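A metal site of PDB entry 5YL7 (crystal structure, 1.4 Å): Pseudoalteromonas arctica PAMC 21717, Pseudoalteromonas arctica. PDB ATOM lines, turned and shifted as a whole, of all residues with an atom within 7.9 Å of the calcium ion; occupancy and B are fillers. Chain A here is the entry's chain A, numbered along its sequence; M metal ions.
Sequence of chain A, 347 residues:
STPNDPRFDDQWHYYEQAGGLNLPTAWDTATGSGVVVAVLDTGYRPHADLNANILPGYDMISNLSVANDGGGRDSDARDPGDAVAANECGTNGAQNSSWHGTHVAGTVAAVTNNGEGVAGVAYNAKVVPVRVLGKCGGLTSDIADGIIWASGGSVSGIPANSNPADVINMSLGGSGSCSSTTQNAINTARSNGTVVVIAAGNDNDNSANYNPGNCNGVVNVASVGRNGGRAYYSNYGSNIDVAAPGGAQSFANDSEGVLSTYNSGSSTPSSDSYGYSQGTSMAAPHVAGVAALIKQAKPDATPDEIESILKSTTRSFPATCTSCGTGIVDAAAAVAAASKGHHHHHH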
ATOM      1  N   PRO A   3      -0.857  16.061  13.730  1.00  0.00           N
ATOM      2  CA  PRO A   3      -1.730  15.988  14.851  1.00  0.00           C
ATOM      3  C   PRO A   3      -1.609  17.099  15.855  1.00  0.00           C
ATOM      4  O   PRO A   3      -0.641  17.777  15.868  1.00  0.00           O
ATOM      5  CB  PRO A   3      -1.445  14.639  15.416  1.00  0.00           C
ATOM      6  CG  PRO A   3      -0.065  14.411  15.112  1.00  0.00           C
ATOM      7  CD  PRO A   3       0.214  15.042  13.745  1.00  0.00           C
ATOM      8  N   ASN A   4      -2.614  17.146  16.699  1.00  0.00           N
ATOM      9  CA  ASN A   4      -2.674  18.184  17.682  1.00  0.00           C
ATOM     10  C   ASN A   4      -2.028  17.950  19.044  1.00  0.00           C
ATOM     11  O   ASN A   4      -1.943  18.750  19.924  1.00  0.00           O
ATOM     12  CB  ASN A   4      -4.149  18.605  17.903  1.00  0.00           C
ATOM     13  CG  ASN A   4      -4.903  17.654  18.722  1.00  0.00           C
ATOM     14  OD1 ASN A   4      -4.409  16.699  19.347  1.00  0.00           O
ATOM     15  ND2 ASN A   4      -6.188  17.993  18.965  1.00  0.00           N
ATOM     16  N   ASP A   5      -1.343  16.769  19.128  1.00  0.00           N
ATOM     17  CA  ASP A   5      -0.750  16.421  20.399  1.00  0.00           C
ATOM     18  C   ASP A   5       0.343  17.420  20.800  1.00  0.00           C
ATOM     19  O   ASP A   5       1.199  17.692  19.959  1.00  0.00           O
ATOM     20  CB  ASP A   5      -0.236  14.967  20.319  1.00  0.00           C
ATOM     21  CG  ASP A   5      -1.297  14.016  19.860  1.00  0.00           C
ATOM     22  OD1 ASP A   5      -1.588  14.028  18.663  1.00  0.00           O
ATOM     23  OD2 ASP A   5      -1.926  13.306  20.663  1.00  0.00           O
ATOM     24  N   PRO A   6       0.357  17.877  22.046  1.00  0.00           N
ATOM     25  CA  PRO A   6       1.222  18.999  22.372  1.00  0.00           C
ATOM     26  C   PRO A   6       2.687  18.654  22.352  1.00  0.00           C
ATOM     27  O   PRO A   6       3.524  19.532  22.215  1.00  0.00           O
ATOM     28  CB  PRO A   6       0.769  19.403  23.768  1.00  0.00           C
ATOM     29  CG  PRO A   6       0.035  18.134  24.274  1.00  0.00           C
ATOM     30  CD  PRO A   6      -0.636  17.566  23.118  1.00  0.00           C
ATOM     31  N   ARG A   7       3.075  17.382  22.530  1.00  0.00           N
ATOM     32  CA  ARG A   7       4.461  16.991  22.400  1.00  0.00           C
ATOM     33  C   ARG A   7       4.887  16.563  21.010  1.00  0.00           C
ATOM     34  O   ARG A   7       6.059  16.167  20.823  1.00  0.00           O
ATOM     35  CB  ARG A   7       4.801  15.896  23.422  1.00  0.00           C
ATOM     36  CG  ARG A   7       4.551  16.276  24.841  1.00  0.00           C
ATOM     37  CD  ARG A   7       5.373  17.373  25.325  1.00  0.00           C
ATOM     38  NE  ARG A   7       6.763  17.057  25.427  1.00  0.00           N
ATOM     39  CZ  ARG A   7       7.370  16.453  26.400  1.00  0.00           C
ATOM     40  NH1 ARG A   7       6.732  15.965  27.454  1.00  0.00           N
ATOM     41  NH2 ARG A   7       8.698  16.274  26.328  1.00  0.00           N
ATOM     42  N   PHE A   8       4.038  16.603  20.010  1.00  0.00           N
ATOM     43  CA  PHE A   8       4.400  16.240  18.635  1.00  0.00           C
ATOM     44  C   PHE A   8       5.601  16.962  18.172  1.00  0.00           C
ATOM     45  O   PHE A   8       6.494  16.373  17.566  1.00  0.00           O
ATOM     46  CB  PHE A   8       3.240  16.454  17.678  1.00  0.00           C
ATOM     47  CG  PHE A   8       3.580  16.125  16.270  1.00  0.00           C
ATOM     48  CD1 PHE A   8       3.681  14.827  15.799  1.00  0.00           C
ATOM     49  CD2 PHE A   8       3.867  17.167  15.405  1.00  0.00           C
ATOM     50  CE1 PHE A   8       4.043  14.624  14.475  1.00  0.00           C
ATOM     51  CE2 PHE A   8       4.210  16.954  14.128  1.00  0.00           C
ATOM     52  CZ  PHE A   8       4.313  15.698  13.650  1.00  0.00           C
ATOM     53  N   GLN A  11       8.765  15.382  18.936  1.00  0.00           N
ATOM     54  CA  GLN A  11       8.975  14.088  18.284  1.00  0.00           C
ATOM     55  C   GLN A  11       9.537  14.321  16.879  1.00  0.00           C
ATOM     56  O   GLN A  11       9.007  14.017  15.869  1.00  0.00           O
ATOM     57  CB  GLN A  11       7.642  13.305  18.230  1.00  0.00           C
ATOM     58  CG  GLN A  11       7.184  12.918  19.634  1.00  0.00           C
ATOM     59  CD  GLN A  11       5.960  12.086  19.651  1.00  0.00           C
ATOM     60  OE1 GLN A  11       4.858  12.514  19.276  1.00  0.00           O
ATOM     61  NE2 GLN A  11       6.115  10.803  20.041  1.00  0.00           N
ATOM     62  N   HIS A  47      -1.075   3.582  30.271  1.00  0.00           N
ATOM     63  CA  HIS A  47      -0.839   5.045  30.201  1.00  0.00           C
ATOM     64  C   HIS A  47      -2.073   5.671  29.582  1.00  0.00           C
ATOM     65  O   HIS A  47      -2.617   5.172  28.578  1.00  0.00           O
ATOM     66  CB  HIS A  47       0.447   5.274  29.365  1.00  0.00           C
ATOM     67  CG  HIS A  47       0.945   6.681  29.374  1.00  0.00           C
ATOM     68  ND1 HIS A  47       0.222   7.756  28.883  1.00  0.00           N
ATOM     69  CD2 HIS A  47       2.167   7.120  29.723  1.00  0.00           C
ATOM     70  CE1 HIS A  47       1.023   8.819  28.978  1.00  0.00           C
ATOM     71  NE2 HIS A  47       2.205   8.443  29.475  1.00  0.00           N
ATOM     72  N   ALA A  48      -2.445   6.798  30.110  1.00  0.00           N
ATOM     73  CA  ALA A  48      -3.586   7.543  29.570  1.00  0.00           C
ATOM     74  C   ALA A  48      -3.539   7.877  28.116  1.00  0.00           C
ATOM     75  O   ALA A  48      -4.539   8.017  27.410  1.00  0.00           O
ATOM     76  CB  ALA A  48      -3.796   8.866  30.342  1.00  0.00           C
ATOM     77  N   ASP A  49      -2.260   8.006  27.579  1.00  0.00           N
ATOM     78  CA  ASP A  49      -2.063   8.318  26.165  1.00  0.00           C
ATOM     79  C   ASP A  49      -1.781   7.113  25.273  1.00  0.00           C
ATOM     80  O   ASP A  49      -1.300   7.225  24.181  1.00  0.00           O
ATOM     81  CB  ASP A  49      -0.971   9.388  25.954  1.00  0.00           C
ATOM     82  CG  ASP A  49      -1.163  10.269  24.778  1.00  0.00           C
ATOM     83  OD1 ASP A  49      -2.337  10.554  24.415  1.00  0.00           O
ATOM     84  OD2 ASP A  49      -0.138  10.725  24.172  1.00  0.00           O
ATOM     85  N   LEU A  50      -2.082   5.926  25.847  1.00  0.00           N
ATOM     86  CA  LEU A  50      -1.825   4.633  25.129  1.00  0.00           C
ATOM     87  C   LEU A  50      -3.006   3.680  25.241  1.00  0.00           C
ATOM     88  O   LEU A  50      -3.269   2.922  24.295  1.00  0.00           O
ATOM     89  CB  LEU A  50      -0.555   4.004  25.758  1.00  0.00           C
ATOM     90  CG  LEU A  50      -0.101   2.689  25.143  1.00  0.00           C
ATOM     91  CD1 LEU A  50       0.192   2.858  23.642  1.00  0.00           C
ATOM     92  CD2 LEU A  50       1.055   2.156  25.923  1.00  0.00           C
ATOM     93  N   ALA A 110       0.657   5.245  20.199  1.00  0.00           N
ATOM     94  CA  ALA A 110       0.121   6.208  21.160  1.00  0.00           C
ATOM     95  C   ALA A 110      -1.136   6.824  20.538  1.00  0.00           C
ATOM     96  O   ALA A 110      -1.258   7.073  19.348  1.00  0.00           O
ATOM     97  CB  ALA A 110       1.079   7.289  21.513  1.00  0.00           C
ATOM     98  N   VAL A 111      -2.057   7.139  21.472  1.00  0.00           N
ATOM     99  CA  VAL A 111      -3.316   7.780  21.085  1.00  0.00           C
ATOM    100  C   VAL A 111      -3.032   9.182  20.583  1.00  0.00           C
ATOM    101  O   VAL A 111      -2.346   9.937  21.266  1.00  0.00           O
ATOM    102  CB  VAL A 111      -4.269   7.782  22.248  1.00  0.00           C
ATOM    103  CG1 VAL A 111      -5.579   8.535  21.796  1.00  0.00           C
ATOM    104  CG2 VAL A 111      -4.628   6.399  22.790  1.00  0.00           C
ATOM    105  N   THR A 112      -3.473   9.485  19.396  1.00  0.00           N
ATOM    106  CA  THR A 112      -3.085  10.666  18.664  1.00  0.00           C
ATOM    107  C   THR A 112      -4.358  11.535  18.397  1.00  0.00           C
ATOM    108  O   THR A 112      -5.451  11.035  18.270  1.00  0.00           O
ATOM    109  CB  THR A 112      -2.368  10.218  17.397  1.00  0.00           C
ATOM    110  OG1 THR A 112      -1.190   9.489  17.832  1.00  0.00           O
ATOM    111  CG2 THR A 112      -1.890  11.329  16.523  1.00  0.00           C
ATOM    112  N   ASN A 113      -4.063  12.835  18.275  1.00  0.00           N
ATOM    113  CA  ASN A 113      -5.166  13.839  18.054  1.00  0.00           C
ATOM    114  C   ASN A 113      -6.044  13.886  19.183  1.00  0.00           C
ATOM    115  O   ASN A 113      -7.233  14.282  19.011  1.00  0.00           O
ATOM    116  CB  ASN A 113      -5.910  13.555  16.767  1.00  0.00           C
ATOM    117  CG  ASN A 113      -5.222  14.149  15.672  1.00  0.00           C
ATOM    118  OD1 ASN A 113      -4.800  15.318  15.752  1.00  0.00           O
ATOM    119  ND2 ASN A 113      -5.203  13.412  14.557  1.00  0.00           N
ATOM    120  N   ASN A 114      -5.608  13.589  20.391  1.00  0.00           N
ATOM    121  CA  ASN A 114      -6.379  13.692  21.625  1.00  0.00           C
ATOM    122  C   ASN A 114      -5.980  14.879  22.487  1.00  0.00           C
ATOM    123  O   ASN A 114      -6.312  14.957  23.651  1.00  0.00           O
ATOM    124  CB  ASN A 114      -6.411  12.379  22.426  1.00  0.00           C
ATOM    125  CG  ASN A 114      -5.021  11.999  22.977  1.00  0.00           C
ATOM    126  OD1 ASN A 114      -3.986  12.480  22.461  1.00  0.00           O
ATOM    127  ND2 ASN A 114      -4.990  11.222  24.023  1.00  0.00           N
ATOM    128  N   GLY A 115      -5.154  15.782  21.938  1.00  0.00           N
ATOM    129  CA  GLY A 115      -4.786  16.944  22.662  1.00  0.00           C
ATOM    130  C   GLY A 115      -3.948  16.802  23.843  1.00  0.00           C
ATOM    131  O   GLY A 115      -3.777  17.675  24.723  1.00  0.00           O
ATOM    132  N   GLU A 116      -3.297  15.587  23.962  1.00  0.00           N
ATOM    133  CA  GLU A 116      -2.594  15.169  25.140  1.00  0.00           C
ATOM    134  C   GLU A 116      -1.263  14.472  24.724  1.00  0.00           C
ATOM    135  O   GLU A 116      -1.336  13.683  23.781  1.00  0.00           O
ATOM    136  CB  GLU A 116      -3.412  14.148  25.949  1.00  0.00           C
ATOM    137  CG  GLU A 116      -2.810  13.708  27.229  1.00  0.00           C
ATOM    138  CD  GLU A 116      -3.779  12.807  28.043  1.00  0.00           C
ATOM    139  OE1 GLU A 116      -3.293  12.316  29.096  1.00  0.00           O
ATOM    140  OE2 GLU A 116      -4.956  12.584  27.580  1.00  0.00           O
ATOM    141  N   GLY A 117      -0.193  14.746  25.386  1.00  0.00           N
ATOM    142  CA  GLY A 117       1.003  13.868  25.244  1.00  0.00           C
ATOM    143  C   GLY A 117       1.505  13.882  23.827  1.00  0.00           C
ATOM    144  O   GLY A 117       1.715  14.915  23.161  1.00  0.00           O
ATOM    145  N   VAL A 118       1.813  12.668  23.347  1.00  0.00           N
ATOM    146  CA  VAL A 118       2.485  12.343  22.112  1.00  0.00           C
ATOM    147  C   VAL A 118       1.636  11.784  21.003  1.00  0.00           C
ATOM    148  O   VAL A 118       0.408  11.523  21.264  1.00  0.00           O
ATOM    149  CB  VAL A 118       3.692  11.352  22.420  1.00  0.00           C
ATOM    150  CG1 VAL A 118       4.730  11.997  23.312  1.00  0.00           C
ATOM    151  CG2 VAL A 118       3.157  10.104  23.047  1.00  0.00           C
ATOM    152  N   ALA A 119       2.230  11.533  19.836  1.00  0.00           N
ATOM    153  CA  ALA A 119       1.613  10.802  18.788  1.00  0.00           C
ATOM    154  C   ALA A 119       2.292   9.463  18.572  1.00  0.00           C
ATOM    155  O   ALA A 119       3.407   9.237  19.080  1.00  0.00           O
ATOM    156  CB  ALA A 119       1.617  11.636  17.512  1.00  0.00           C
ATOM    157  N   GLY A 120       1.588   8.594  17.878  1.00  0.00           N
ATOM    158  CA  GLY A 120       2.106   7.282  17.500  1.00  0.00           C
ATOM    159  C   GLY A 120       2.241   7.192  16.018  1.00  0.00           C
ATOM    160  O   GLY A 120       1.569   7.881  15.225  1.00  0.00           O
ATOM    161  N   THR A 261       5.535   7.479  25.384  1.00  0.00           N
ATOM    162  CA  THR A 261       4.894   7.136  26.673  1.00  0.00           C
ATOM    163  C   THR A 261       5.796   6.451  27.578  1.00  0.00           C
ATOM    164  O   THR A 261       6.615   5.570  27.143  1.00  0.00           O
ATOM    165  CB  THR A 261       3.625   6.312  26.407  1.00  0.00           C
ATOM    166  OG1 THR A 261       3.897   5.289  25.412  1.00  0.00           O
ATOM    167  CG2 THR A 261       2.520   7.170  25.807  1.00  0.00           C
ATOM    168  N   TYR A 274       6.199  11.032  30.125  1.00  0.00           N
ATOM    169  CA  TYR A 274       6.756  10.957  28.779  1.00  0.00           C
ATOM    170  C   TYR A 274       8.199  11.023  28.870  1.00  0.00           C
ATOM    171  O   TYR A 274       8.729  11.813  29.698  1.00  0.00           O
ATOM    172  CB  TYR A 274       6.214  12.055  27.872  1.00  0.00           C
ATOM    173  CG  TYR A 274       4.716  12.075  27.792  1.00  0.00           C
ATOM    174  CD1 TYR A 274       3.990  11.215  26.982  1.00  0.00           C
ATOM    175  CD2 TYR A 274       3.956  12.951  28.612  1.00  0.00           C
ATOM    176  CE1 TYR A 274       2.608  11.156  27.021  1.00  0.00           C
ATOM    177  CE2 TYR A 274       2.579  12.835  28.648  1.00  0.00           C
ATOM    178  CZ  TYR A 274       1.930  12.000  27.792  1.00  0.00           C
ATOM    179  OH  TYR A 274       0.555  11.893  27.783  1.00  0.00           O
HETATM  180 CA    CA M   1      -1.630  11.788  22.442  1.00  0.00          CA
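Six residues have an atom within 4 Å of the calcium ion: Asp 5, Asp 49, Val 111, Asn 114, Glu 116 and Val 118.
N of Asn 114 lies within hydrogen-bond range of OD1 of Asn 4 (3.5 Å).
A ring nitrogen (ND1) of His 47 lies within hydrogen-bond range of the backbone NH of Asp 49 (2.8 Å).
The side-chain carboxylate (OD1) of Asp 5 lies within hydrogen-bond range of the backbone NH (N) of Asn 113, at 2.8 Å.
The calcium ion is bound by O of Val 111 (2.3 Å), O of Glu 116 (2.3 Å), OD2 of Asp 5 (2.4 Å), O of Val 118 (2.4 Å), OD1 of Asp 49 (2.4 Å), OD1 of Asn 114 (2.5 Å) and OD2 of Asp 49 (2.5 Å).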
